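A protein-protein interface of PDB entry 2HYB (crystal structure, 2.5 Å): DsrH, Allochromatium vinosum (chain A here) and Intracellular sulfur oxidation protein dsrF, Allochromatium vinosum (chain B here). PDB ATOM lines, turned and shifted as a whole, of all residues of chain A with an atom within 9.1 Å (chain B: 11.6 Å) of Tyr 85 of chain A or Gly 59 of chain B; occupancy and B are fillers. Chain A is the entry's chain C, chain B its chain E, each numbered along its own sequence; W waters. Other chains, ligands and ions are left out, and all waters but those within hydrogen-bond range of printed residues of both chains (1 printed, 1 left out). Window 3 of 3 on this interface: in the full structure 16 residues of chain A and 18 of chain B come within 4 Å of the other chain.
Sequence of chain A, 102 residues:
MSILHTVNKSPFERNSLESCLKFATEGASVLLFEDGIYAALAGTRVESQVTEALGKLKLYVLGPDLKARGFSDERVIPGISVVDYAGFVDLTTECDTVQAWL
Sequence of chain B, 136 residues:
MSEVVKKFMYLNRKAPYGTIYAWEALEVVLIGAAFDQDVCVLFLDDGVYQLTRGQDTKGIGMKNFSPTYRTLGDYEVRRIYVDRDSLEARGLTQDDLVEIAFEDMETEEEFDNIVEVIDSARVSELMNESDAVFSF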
ATOM      1  N   LEU A  31     -18.886  30.180 -19.416  1.00  0.00           N
ATOM      2  CA  LEU A  31     -19.769  29.650 -18.390  1.00  0.00           C
ATOM      3  C   LEU A  31     -20.482  30.783 -17.658  1.00  0.00           C
ATOM      4  O   LEU A  31     -19.840  31.682 -17.116  1.00  0.00           O
ATOM      5  CB  LEU A  31     -18.956  28.824 -17.404  1.00  0.00           C
ATOM      6  CG  LEU A  31     -19.603  28.485 -16.062  1.00  0.00           C
ATOM      7  CD1 LEU A  31     -20.930  27.778 -16.301  1.00  0.00           C
ATOM      8  CD2 LEU A  31     -18.661  27.611 -15.243  1.00  0.00           C
ATOM      9  N   PHE A  33     -22.586  31.907 -14.528  1.00  0.00           N
ATOM     10  CA  PHE A  33     -22.977  31.492 -13.188  1.00  0.00           C
ATOM     11  C   PHE A  33     -23.279  32.718 -12.314  1.00  0.00           C
ATOM     12  O   PHE A  33     -23.128  33.862 -12.767  1.00  0.00           O
ATOM     13  CB  PHE A  33     -21.919  30.561 -12.572  1.00  0.00           C
ATOM     14  CG  PHE A  33     -20.663  31.252 -12.102  1.00  0.00           C
ATOM     15  CD1 PHE A  33     -19.826  31.926 -12.993  1.00  0.00           C
ATOM     16  CD2 PHE A  33     -20.310  31.210 -10.751  1.00  0.00           C
ATOM     17  CE1 PHE A  33     -18.662  32.545 -12.548  1.00  0.00           C
ATOM     18  CE2 PHE A  33     -19.150  31.826 -10.300  1.00  0.00           C
ATOM     19  CZ  PHE A  33     -18.326  32.496 -11.204  1.00  0.00           C
ATOM     20  N   GLU A  34     -23.721  32.487 -11.079  1.00  0.00           N
ATOM     21  CA  GLU A  34     -24.118  33.586 -10.192  1.00  0.00           C
ATOM     22  C   GLU A  34     -25.116  34.452 -10.975  1.00  0.00           C
ATOM     23  O   GLU A  34     -25.894  33.922 -11.758  1.00  0.00           O
ATOM     24  CB  GLU A  34     -22.902  34.386  -9.729  1.00  0.00           C
ATOM     25  CG  GLU A  34     -22.163  33.700  -8.577  1.00  0.00           C
ATOM     26  CD  GLU A  34     -20.996  34.511  -8.023  1.00  0.00           C
ATOM     27  OE1 GLU A  34     -20.964  35.744  -8.241  1.00  0.00           O
ATOM     28  OE2 GLU A  34     -20.124  33.915  -7.347  1.00  0.00           O
ATOM     29  N   ILE A  37     -26.303  34.052 -14.843  1.00  0.00           N
ATOM     30  CA  ILE A  37     -27.355  33.155 -15.295  1.00  0.00           C
ATOM     31  C   ILE A  37     -28.457  33.775 -16.163  1.00  0.00           C
ATOM     32  O   ILE A  37     -28.848  33.204 -17.176  1.00  0.00           O
ATOM     33  CB  ILE A  37     -27.984  32.446 -14.053  1.00  0.00           C
ATOM     34  CG1 ILE A  37     -27.633  30.972 -14.113  1.00  0.00           C
ATOM     35  CG2 ILE A  37     -29.495  32.684 -13.951  1.00  0.00           C
ATOM     36  CD1 ILE A  37     -26.168  30.722 -14.011  1.00  0.00           C
ATOM     37  N   VAL A  61     -24.209  27.209 -18.529  1.00  0.00           N
ATOM     38  CA  VAL A  61     -24.822  27.946 -17.439  1.00  0.00           C
ATOM     39  C   VAL A  61     -24.862  26.988 -16.246  1.00  0.00           C
ATOM     40  O   VAL A  61     -25.078  25.784 -16.426  1.00  0.00           O
ATOM     41  CB  VAL A  61     -26.236  28.423 -17.859  1.00  0.00           C
ATOM     42  CG1 VAL A  61     -27.110  27.238 -18.209  1.00  0.00           C
ATOM     43  CG2 VAL A  61     -26.852  29.262 -16.771  1.00  0.00           C
ATOM     44  N   LEU A  62     -24.626  27.505 -15.039  1.00  0.00           N
ATOM     45  CA  LEU A  62     -24.607  26.676 -13.826  1.00  0.00           C
ATOM     46  C   LEU A  62     -26.009  26.397 -13.297  1.00  0.00           C
ATOM     47  O   LEU A  62     -26.732  27.311 -12.893  1.00  0.00           O
ATOM     48  CB  LEU A  62     -23.778  27.365 -12.743  1.00  0.00           C
ATOM     49  CG  LEU A  62     -23.450  26.540 -11.501  1.00  0.00           C
ATOM     50  CD1 LEU A  62     -22.540  25.390 -11.887  1.00  0.00           C
ATOM     51  CD2 LEU A  62     -22.775  27.433 -10.462  1.00  0.00           C
ATOM     52  N   GLY A  63     -26.386  25.126 -13.299  1.00  0.00           N
ATOM     53  CA  GLY A  63     -27.711  24.744 -12.842  1.00  0.00           C
ATOM     54  C   GLY A  63     -28.124  25.357 -11.518  1.00  0.00           C
ATOM     55  O   GLY A  63     -29.110  26.098 -11.456  1.00  0.00           O
ATOM     56  N   PRO A  64     -27.378  25.061 -10.439  1.00  0.00           N
ATOM     57  CA  PRO A  64     -27.646  25.570  -9.092  1.00  0.00           C
ATOM     58  C   PRO A  64     -28.080  27.046  -9.063  1.00  0.00           C
ATOM     59  O   PRO A  64     -29.023  27.406  -8.344  1.00  0.00           O
ATOM     60  CB  PRO A  64     -26.325  25.324  -8.375  1.00  0.00           C
ATOM     61  CG  PRO A  64     -25.838  24.057  -9.026  1.00  0.00           C
ATOM     62  CD  PRO A  64     -26.101  24.321 -10.476  1.00  0.00           C
ATOM     63  N   ASP A  65     -27.412  27.902  -9.840  1.00  0.00           N
ATOM     64  CA  ASP A  65     -27.778  29.318  -9.863  1.00  0.00           C
ATOM     65  C   ASP A  65     -29.006  29.613 -10.694  1.00  0.00           C
ATOM     66  O   ASP A  65     -29.668  30.623 -10.479  1.00  0.00           O
ATOM     67  CB  ASP A  65     -26.622  30.185 -10.359  1.00  0.00           C
ATOM     68  CG  ASP A  65     -25.600  30.453  -9.278  1.00  0.00           C
ATOM     69  OD1 ASP A  65     -26.007  30.835  -8.157  1.00  0.00           O
ATOM     70  OD2 ASP A  65     -24.391  30.283  -9.552  1.00  0.00           O
ATOM     71  N   LEU A  66     -29.302  28.762 -11.666  1.00  0.00           N
ATOM     72  CA  LEU A  66     -30.498  28.977 -12.464  1.00  0.00           C
ATOM     73  C   LEU A  66     -31.687  28.692 -11.553  1.00  0.00           C
ATOM     74  O   LEU A  66     -32.621  29.490 -11.464  1.00  0.00           O
ATOM     75  CB  LEU A  66     -30.544  28.016 -13.647  1.00  0.00           C
ATOM     76  CG  LEU A  66     -30.012  28.501 -14.994  1.00  0.00           C
ATOM     77  CD1 LEU A  66     -30.065  27.346 -15.965  1.00  0.00           C
ATOM     78  CD2 LEU A  66     -30.832  29.677 -15.513  1.00  0.00           C
ATOM     79  N   LYS A  67     -31.633  27.556 -10.868  1.00  0.00           N
ATOM     80  CA  LYS A  67     -32.705  27.141  -9.976  1.00  0.00           C
ATOM     81  C   LYS A  67     -32.920  28.111  -8.839  1.00  0.00           C
ATOM     82  O   LYS A  67     -34.045  28.493  -8.558  1.00  0.00           O
ATOM     83  CB  LYS A  67     -32.406  25.756  -9.401  1.00  0.00           C
ATOM     84  CG  LYS A  67     -32.079  24.722 -10.457  1.00  0.00           C
ATOM     85  CD  LYS A  67     -31.817  23.359  -9.839  1.00  0.00           C
ATOM     86  CE  LYS A  67     -31.124  22.436 -10.824  1.00  0.00           C
ATOM     87  NZ  LYS A  67     -31.863  22.310 -12.103  1.00  0.00           N
ATOM     88  N   ALA A  68     -31.835  28.500  -8.181  1.00  0.00           N
ATOM     89  CA  ALA A  68     -31.917  29.418  -7.053  1.00  0.00           C
ATOM     90  C   ALA A  68     -32.645  30.696  -7.441  1.00  0.00           C
ATOM     91  O   ALA A  68     -33.323  31.311  -6.609  1.00  0.00           O
ATOM     92  CB  ALA A  68     -30.511  29.744  -6.540  1.00  0.00           C
ATOM     93  N   ARG A  69     -32.508  31.098  -8.704  1.00  0.00           N
ATOM     94  CA  ARG A  69     -33.161  32.317  -9.164  1.00  0.00           C
ATOM     95  C   ARG A  69     -34.555  32.095  -9.733  1.00  0.00           C
ATOM     96  O   ARG A  69     -35.226  33.047 -10.150  1.00  0.00           O
ATOM     97  CB  ARG A  69     -32.244  33.052 -10.148  1.00  0.00           C
ATOM     98  CG  ARG A  69     -31.008  33.565  -9.427  1.00  0.00           C
ATOM     99  CD  ARG A  69     -30.001  34.309 -10.275  1.00  0.00           C
ATOM    100  NE  ARG A  69     -28.867  34.722  -9.452  1.00  0.00           N
ATOM    101  CZ  ARG A  69     -28.001  33.878  -8.893  1.00  0.00           C
ATOM    102  NH1 ARG A  69     -28.127  32.567  -9.071  1.00  0.00           N
ATOM    103  NH2 ARG A  69     -27.009  34.342  -8.141  1.00  0.00           N
ATOM    104  N   VAL A  82     -26.409  23.030 -19.532  1.00  0.00           N
ATOM    105  CA  VAL A  82     -26.507  23.235 -18.098  1.00  0.00           C
ATOM    106  C   VAL A  82     -25.577  22.271 -17.350  1.00  0.00           C
ATOM    107  O   VAL A  82     -25.633  21.054 -17.558  1.00  0.00           O
ATOM    108  CB  VAL A  82     -27.938  22.999 -17.606  1.00  0.00           C
ATOM    109  CG1 VAL A  82     -27.993  23.146 -16.094  1.00  0.00           C
ATOM    110  CG2 VAL A  82     -28.892  23.983 -18.272  1.00  0.00           C
ATOM    111  N   VAL A  83     -24.732  22.823 -16.479  1.00  0.00           N
ATOM    112  CA  VAL A  83     -23.797  22.026 -15.687  1.00  0.00           C
ATOM    113  C   VAL A  83     -23.909  22.378 -14.192  1.00  0.00           C
ATOM    114  O   VAL A  83     -24.415  23.452 -13.839  1.00  0.00           O
ATOM    115  CB  VAL A  83     -22.328  22.275 -16.143  1.00  0.00           C
ATOM    116  CG1 VAL A  83     -22.189  22.011 -17.622  1.00  0.00           C
ATOM    117  CG2 VAL A  83     -21.907  23.709 -15.821  1.00  0.00           C
ATOM    118  N   ASP A  84     -23.447  21.472 -13.324  1.00  0.00           N
ATOM    119  CA  ASP A  84     -23.462  21.701 -11.872  1.00  0.00           C
ATOM    120  C   ASP A  84     -22.027  21.992 -11.423  1.00  0.00           C
ATOM    121  O   ASP A  84     -21.136  22.111 -12.268  1.00  0.00           O
ATOM    122  CB  ASP A  84     -24.012  20.477 -11.130  1.00  0.00           C
ATOM    123  CG  ASP A  84     -23.243  19.200 -11.440  1.00  0.00           C
ATOM    124  OD1 ASP A  84     -22.075  19.276 -11.884  1.00  0.00           O
ATOM    125  OD2 ASP A  84     -23.806  18.107 -11.219  1.00  0.00           O
ATOM    126  N   TYR A  85     -21.784  22.115 -10.121  1.00  0.00           N
ATOM    127  CA  TYR A  85     -20.421  22.405  -9.685  1.00  0.00           C
ATOM    128  C   TYR A  85     -19.437  21.347 -10.124  1.00  0.00           C
ATOM    129  O   TYR A  85     -18.294  21.656 -10.449  1.00  0.00           O
ATOM    130  CB  TYR A  85     -20.340  22.585  -8.171  1.00  0.00           C
ATOM    131  CG  TYR A  85     -20.935  23.890  -7.721  1.00  0.00           C
ATOM    132  CD1 TYR A  85     -22.159  23.925  -7.055  1.00  0.00           C
ATOM    133  CD2 TYR A  85     -20.309  25.096  -8.019  1.00  0.00           C
ATOM    134  CE1 TYR A  85     -22.743  25.127  -6.698  1.00  0.00           C
ATOM    135  CE2 TYR A  85     -20.887  26.306  -7.676  1.00  0.00           C
ATOM    136  CZ  TYR A  85     -22.103  26.319  -7.015  1.00  0.00           C
ATOM    137  OH  TYR A  85     -22.681  27.525  -6.678  1.00  0.00           O
ATOM    138  N   ALA A  86     -19.862  20.093 -10.136  1.00  0.00           N
ATOM    139  CA  ALA A  86     -18.958  19.044 -10.580  1.00  0.00           C
ATOM    140  C   ALA A  86     -18.586  19.339 -12.044  1.00  0.00           C
ATOM    141  O   ALA A  86     -17.427  19.228 -12.439  1.00  0.00           O
ATOM    142  CB  ALA A  86     -19.629  17.696 -10.460  1.00  0.00           C
ATOM    143  N   GLY A  87     -19.578  19.736 -12.839  1.00  0.00           N
ATOM    144  CA  GLY A  87     -19.333  20.045 -14.238  1.00  0.00           C
ATOM    145  C   GLY A  87     -18.489  21.297 -14.410  1.00  0.00           C
ATOM    146  O   GLY A  87     -17.653  21.391 -15.314  1.00  0.00           O
ATOM    147  N   PHE A  88     -18.725  22.271 -13.542  1.00  0.00           N
ATOM    148  CA  PHE A  88     -17.981  23.515 -13.569  1.00  0.00           C
ATOM    149  C   PHE A  88     -16.512  23.129 -13.398  1.00  0.00           C
ATOM    150  O   PHE A  88     -15.642  23.586 -14.146  1.00  0.00           O
ATOM    151  CB  PHE A  88     -18.477  24.411 -12.427  1.00  0.00           C
ATOM    152  CG  PHE A  88     -17.814  25.765 -12.350  1.00  0.00           C
ATOM    153  CD1 PHE A  88     -18.364  26.762 -11.537  1.00  0.00           C
ATOM    154  CD2 PHE A  88     -16.633  26.040 -13.035  1.00  0.00           C
ATOM    155  CE1 PHE A  88     -17.746  28.011 -11.404  1.00  0.00           C
ATOM    156  CE2 PHE A  88     -16.007  27.278 -12.912  1.00  0.00           C
ATOM    157  CZ  PHE A  88     -16.565  28.267 -12.093  1.00  0.00           C
ATOM    158  N   VAL A  89     -16.240  22.270 -12.422  1.00  0.00           N
ATOM    159  CA  VAL A  89     -14.873  21.822 -12.184  1.00  0.00           C
ATOM    160  C   VAL A  89     -14.327  21.240 -13.482  1.00  0.00           C
ATOM    161  O   VAL A  89     -13.267  21.642 -13.954  1.00  0.00           O
ATOM    162  CB  VAL A  89     -14.814  20.734 -11.090  1.00  0.00           C
ATOM    163  CG1 VAL A  89     -13.395  20.174 -10.970  1.00  0.00           C
ATOM    164  CG2 VAL A  89     -15.275  21.319  -9.758  1.00  0.00           C
ATOM    165  N   ASP A  90     -15.072  20.303 -14.065  1.00  0.00           N
ATOM    166  CA  ASP A  90     -14.662  19.665 -15.310  1.00  0.00           C
ATOM    167  C   ASP A  90     -14.310  20.655 -16.406  1.00  0.00           C
ATOM    168  O   ASP A  90     -13.293  20.505 -17.074  1.00  0.00           O
ATOM    169  CB  ASP A  90     -15.754  18.719 -15.789  1.00  0.00           C
ATOM    170  CG  ASP A  90     -15.821  17.472 -14.956  1.00  0.00           C
ATOM    171  OD1 ASP A  90     -14.735  16.937 -14.643  1.00  0.00           O
ATOM    172  OD2 ASP A  90     -16.939  17.018 -14.621  1.00  0.00           O
ATOM    173  N   LEU A  91     -15.150  21.665 -16.589  1.00  0.00           N
ATOM    174  CA  LEU A  91     -14.888  22.679 -17.598  1.00  0.00           C
ATOM    175  C   LEU A  91     -13.520  23.325 -17.379  1.00  0.00           C
ATOM    176  O   LEU A  91     -12.787  23.571 -18.337  1.00  0.00           O
ATOM    177  CB  LEU A  91     -15.973  23.760 -17.564  1.00  0.00           C
ATOM    178  CG  LEU A  91     -17.343  23.353 -18.102  1.00  0.00           C
ATOM    179  CD1 LEU A  91     -18.295  24.512 -17.944  1.00  0.00           C
ATOM    180  CD2 LEU A  91     -17.226  22.948 -19.572  1.00  0.00           C
ATOM    181  N   THR A  92     -13.173  23.585 -16.120  1.00  0.00           N
ATOM    182  CA  THR A  92     -11.895  24.213 -15.817  1.00  0.00           C
ATOM    183  C   THR A  92     -10.687  23.309 -16.111  1.00  0.00           C
ATOM    184  O   THR A  92      -9.591  23.809 -16.361  1.00  0.00           O
ATOM    185  CB  THR A  92     -11.846  24.748 -14.335  1.00  0.00           C
ATOM    186  OG1 THR A  92     -11.964  23.666 -13.404  1.00  0.00           O
ATOM    187  CG2 THR A  92     -12.977  25.732 -14.090  1.00  0.00           C
ATOM    188  N   PRO B  16     -31.337  38.895  -6.839  1.00  0.00           N
ATOM    189  CA  PRO B  16     -31.105  38.257  -5.540  1.00  0.00           C
ATOM    190  C   PRO B  16     -29.952  37.253  -5.575  1.00  0.00           C
ATOM    191  O   PRO B  16     -29.528  36.817  -6.636  1.00  0.00           O
ATOM    192  CB  PRO B  16     -32.439  37.574  -5.260  1.00  0.00           C
ATOM    193  CG  PRO B  16     -32.851  37.136  -6.622  1.00  0.00           C
ATOM    194  CD  PRO B  16     -32.586  38.392  -7.442  1.00  0.00           C
ATOM    195  N   TYR B  17     -29.455  36.902  -4.393  1.00  0.00           N
ATOM    196  CA  TYR B  17     -28.378  35.928  -4.214  1.00  0.00           C
ATOM    197  C   TYR B  17     -26.994  36.284  -4.774  1.00  0.00           C
ATOM    198  O   TYR B  17     -25.971  35.908  -4.186  1.00  0.00           O
ATOM    199  CB  TYR B  17     -28.826  34.556  -4.740  1.00  0.00           C
ATOM    200  CG  TYR B  17     -30.158  34.099  -4.173  1.00  0.00           C
ATOM    201  CD1 TYR B  17     -31.349  34.337  -4.865  1.00  0.00           C
ATOM    202  CD2 TYR B  17     -30.237  33.464  -2.928  1.00  0.00           C
ATOM    203  CE1 TYR B  17     -32.585  33.956  -4.332  1.00  0.00           C
ATOM    204  CE2 TYR B  17     -31.463  33.083  -2.392  1.00  0.00           C
ATOM    205  CZ  TYR B  17     -32.636  33.331  -3.099  1.00  0.00           C
ATOM    206  OH  TYR B  17     -33.854  32.956  -2.582  1.00  0.00           O
ATOM    207  N   GLY B  18     -26.941  36.981  -5.904  1.00  0.00           N
ATOM    208  CA  GLY B  18     -25.644  37.375  -6.434  1.00  0.00           C
ATOM    209  C   GLY B  18     -25.025  38.250  -5.361  1.00  0.00           C
ATOM    210  O   GLY B  18     -23.826  38.195  -5.095  1.00  0.00           O
ATOM    211  N   GLY B  54     -40.791  30.204  -7.648  1.00  0.00           N
ATOM    212  CA  GLY B  54     -40.138  28.924  -7.854  1.00  0.00           C
ATOM    213  C   GLY B  54     -38.664  28.821  -7.509  1.00  0.00           C
ATOM    214  O   GLY B  54     -38.009  27.848  -7.893  1.00  0.00           O
ATOM    215  N   GLN B  55     -38.123  29.806  -6.800  1.00  0.00           N
ATOM    216  CA  GLN B  55     -36.711  29.741  -6.454  1.00  0.00           C
ATOM    217  C   GLN B  55     -36.423  28.506  -5.609  1.00  0.00           C
ATOM    218  O   GLN B  55     -37.196  28.162  -4.712  1.00  0.00           O
ATOM    219  CB  GLN B  55     -36.290  30.990  -5.681  1.00  0.00           C
ATOM    220  CG  GLN B  55     -36.160  32.254  -6.511  1.00  0.00           C
ATOM    221  CD  GLN B  55     -36.196  33.495  -5.645  1.00  0.00           C
ATOM    222  OE1 GLN B  55     -35.676  33.496  -4.528  1.00  0.00           O
ATOM    223  NE2 GLN B  55     -36.803  34.557  -6.152  1.00  0.00           N
ATOM    224  N   ASP B  56     -35.320  27.832  -5.913  1.00  0.00           N
ATOM    225  CA  ASP B  56     -34.890  26.649  -5.173  1.00  0.00           C
ATOM    226  C   ASP B  56     -33.407  26.864  -4.927  1.00  0.00           C
ATOM    227  O   ASP B  56     -32.589  26.570  -5.799  1.00  0.00           O
ATOM    228  CB  ASP B  56     -35.074  25.378  -5.998  1.00  0.00           C
ATOM    229  CG  ASP B  56     -34.467  24.160  -5.323  1.00  0.00           C
ATOM    230  OD1 ASP B  56     -34.311  23.116  -5.986  1.00  0.00           O
ATOM    231  OD2 ASP B  56     -34.141  24.251  -4.119  1.00  0.00           O
ATOM    232  N   THR B  57     -33.058  27.372  -3.746  1.00  0.00           N
ATOM    233  CA  THR B  57     -31.659  27.646  -3.421  1.00  0.00           C
ATOM    234  C   THR B  57     -30.844  26.465  -2.880  1.00  0.00           C
ATOM    235  O   THR B  57     -29.690  26.629  -2.494  1.00  0.00           O
ATOM    236  CB  THR B  57     -31.544  28.815  -2.410  1.00  0.00           C
ATOM    237  OG1 THR B  57     -32.054  28.413  -1.136  1.00  0.00           O
ATOM    238  CG2 THR B  57     -32.331  30.012  -2.878  1.00  0.00           C
ATOM    239  N   LYS B  58     -31.419  25.270  -2.867  1.00  0.00           N
ATOM    240  CA  LYS B  58     -30.699  24.114  -2.347  1.00  0.00           C
ATOM    241  C   LYS B  58     -29.327  23.915  -2.976  1.00  0.00           C
ATOM    242  O   LYS B  58     -28.336  23.703  -2.277  1.00  0.00           O
ATOM    243  CB  LYS B  58     -31.545  22.849  -2.524  1.00  0.00           C
ATOM    244  CG  LYS B  58     -32.878  22.917  -1.799  1.00  0.00           C
ATOM    245  CD  LYS B  58     -32.679  23.294  -0.340  1.00  0.00           C
ATOM    246  CE  LYS B  58     -33.971  23.767   0.306  1.00  0.00           C
ATOM    247  NZ  LYS B  58     -35.033  22.726   0.274  1.00  0.00           N
ATOM    248  N   GLY B  59     -29.274  24.005  -4.296  1.00  0.00           N
ATOM    249  CA  GLY B  59     -28.029  23.802  -5.007  1.00  0.00           C
ATOM    250  C   GLY B  59     -26.887  24.752  -4.718  1.00  0.00           C
ATOM    251  O   GLY B  59     -25.729  24.362  -4.864  1.00  0.00           O
ATOM    252  N   ILE B  60     -27.174  25.988  -4.320  1.00  0.00           N
ATOM    253  CA  ILE B  60     -26.082  26.905  -4.048  1.00  0.00           C
ATOM    254  C   ILE B  60     -25.742  27.039  -2.566  1.00  0.00           C
ATOM    255  O   ILE B  60     -24.978  27.919  -2.171  1.00  0.00           O
ATOM    256  CB  ILE B  60     -26.336  28.301  -4.689  1.00  0.00           C
ATOM    257  CG1 ILE B  60     -27.495  29.025  -4.004  1.00  0.00           C
ATOM    258  CG2 ILE B  60     -26.598  28.128  -6.169  1.00  0.00           C
ATOM    259  CD1 ILE B  60     -27.622  30.487  -4.407  1.00  0.00           C
ATOM    260  N   GLY B  61     -26.307  26.145  -1.759  1.00  0.00           N
ATOM    261  CA  GLY B  61     -26.046  26.133  -0.326  1.00  0.00           C
ATOM    262  C   GLY B  61     -26.420  27.367   0.476  1.00  0.00           C
ATOM    263  O   GLY B  61     -25.769  27.682   1.466  1.00  0.00           O
ATOM    264  N   MET B  62     -27.461  28.071   0.045  1.00  0.00           N
ATOM    265  CA  MET B  62     -27.935  29.268   0.739  1.00  0.00           C
ATOM    266  C   MET B  62     -29.397  29.056   1.141  1.00  0.00           C
ATOM    267  O   MET B  62     -30.079  28.184   0.598  1.00  0.00           O
ATOM    268  CB  MET B  62     -27.852  30.506  -0.169  1.00  0.00           C
ATOM    269  CG  MET B  62     -26.461  31.038  -0.434  1.00  0.00           C
ATOM    270  SD  MET B  62     -26.524  32.512  -1.476  1.00  0.00           S
ATOM    271  CE  MET B  62     -27.141  33.687  -0.384  1.00  0.00           C
ATOM    272  N   LYS B  63     -29.869  29.853   2.092  1.00  0.00           N
ATOM    273  CA  LYS B  63     -31.250  29.769   2.535  1.00  0.00           C
ATOM    274  C   LYS B  63     -32.085  30.504   1.489  1.00  0.00           C
ATOM    275  O   LYS B  63     -31.655  31.524   0.962  1.00  0.00           O
ATOM    276  CB  LYS B  63     -31.411  30.455   3.895  1.00  0.00           C
ATOM    277  CG  LYS B  63     -32.852  30.521   4.386  1.00  0.00           C
ATOM    278  CD  LYS B  63     -33.022  31.462   5.585  1.00  0.00           C
ATOM    279  CE  LYS B  63     -34.496  31.634   5.932  1.00  0.00           C
ATOM    280  NZ  LYS B  63     -34.749  32.611   7.021  1.00  0.00           N
ATOM    281  N   ASN B  64     -33.260  29.972   1.173  1.00  0.00           N
ATOM    282  CA  ASN B  64     -34.148  30.608   0.209  1.00  0.00           C
ATOM    283  C   ASN B  64     -35.045  31.529   1.017  1.00  0.00           C
ATOM    284  O   ASN B  64     -35.892  31.066   1.772  1.00  0.00           O
ATOM    285  CB  ASN B  64     -34.984  29.554  -0.520  1.00  0.00           C
ATOM    286  CG  ASN B  64     -36.083  30.161  -1.382  1.00  0.00           C
ATOM    287  OD1 ASN B  64     -36.759  29.449  -2.128  1.00  0.00           O
ATOM    288  ND2 ASN B  64     -36.273  31.473  -1.283  1.00  0.00           N
HETATM  289  O   HOH W   1     -22.925  29.514  -4.246  1.00  0.00           O
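O of Pro 64 of chain A touches CG2 of Ile 60 of chain B (3.3 Å).
Ile 60 of chain B touches Asp 65 of chain A (CG2 to OD1, 3.4 Å).
Tyr 17 of chain B touches Ala 68 of chain A (CE1 to O, 3.6 Å).
Ala 68 of chain A touches Gln 55 of chain B.
Ala 68 of chain A touches Thr 57 of chain B.
Pro 16 of chain B touches Arg 69 of chain A (O to NE, 3.6 Å).
Arg 69 of chain A touches Tyr 17 of chain B.
Arg 69 of chain A touches Gln 55 of chain B.
Tyr 85 of chain A touches Gly 59 of chain B.
Ile 60 of chain B touches Tyr 85 of chain A.
Hydrophobic or aromatic side chains of chain B that line the printed part of chain A: Tyr 17 and Ile 60.
Of the 24 printed residues of chain A, 6 touch a printed residue of chain B.
Hydrophobic or aromatic side chains of chain A within 4 Å of the printed part of chain B: Pro 64, Ala 68 and Tyr 85.
Among the printed residues, 16 pairs touch across the chains.
Among the printed residues, no Asp or Glu carboxylate lies within 4 Å of a Lys or Arg side-chain nitrogen of the other chain.
Water W1 bridges the side-chain hydroxyl (OH) of Tyr 85 of chain A and the backbone carbonyl oxygen (O) of Ile 60 of chain B.
Glu 34 of chain A touches none of the printed residues of chain B.
No residue of chain B comes within 4 Å of Gly 63 of chain A.
Of chain B, only Gly 59 (3.7 Å) and Ile 60 (3.3 Å) come within 4 Å of Pro 64 of chain A.
Printed residues of chain B within 4 Å of Lys 67 of chain A: Gln 55 (3.6 Å) and Asp 56 (3.0 Å).
Asp 84 of chain A touches none of the printed residues of chain B.
Printed residues of chain B within 4 Å of Tyr 85 of chain A: Gly 59 and Ile 60.
No residue of chain B comes within 4 Å of Ala 86 of chain A.
No residue of chain B comes within 4 Å of Phe 88 of chain A.
Thr 92 of chain A touches none of the printed residues of chain B.
Of the printed residues of chain A, Asp 56 of chain B touches Lys 67 and Ala 68.
Printed residues of chain A within 4 Å of Thr 57 of chain B: Ala 68 (3.9 Å).
Gly 59 of chain B touches just these residues of chain A: Pro 64 and Tyr 85.
The nearest printed residue of chain A that does not touch Ile 60 of chain B is Arg 69 of chain A (5.1 Å).
OH of Tyr 17 of chain B lies within hydrogen-bond range of OE1 of Gln 55 of chain B (2.7 Å).
The side-chain amide nitrogen of Asn 64 of chain B sits at hydrogen-bond distance from the side-chain hydroxyl of Tyr 17 of chain B.
The backbone NH of Lys 58 of chain B lies close to the side-chain carboxylate of Asp 56 of chain B (3.2 Å).
OG1 of Thr 57 of chain B sits at hydrogen-bond distance from O of Met 62 of chain B (2.6 Å).
N of Asn 64 of chain B lies within hydrogen-bond range of OG1 of Thr 57 of chain B, at 3.0 Å.
OD1 of Asp 65 of chain A is in salt-bridge range of NH1 of Arg 69 of chain A, 2.9 Å away.
O of Lys 67 of chain A lies within hydrogen-bond range of N of Asp 56 of chain B, 3.0 Å away.
The backbone carbonyl oxygen (O) of Asp 56 of chain B is in hydrogen-bond range of the backbone NH (N) of Ala 68 of chain A (3.2 Å).
NH2 of Arg 69 of chain A sits close to N of Gly 18 of chain B (3.5 Å).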
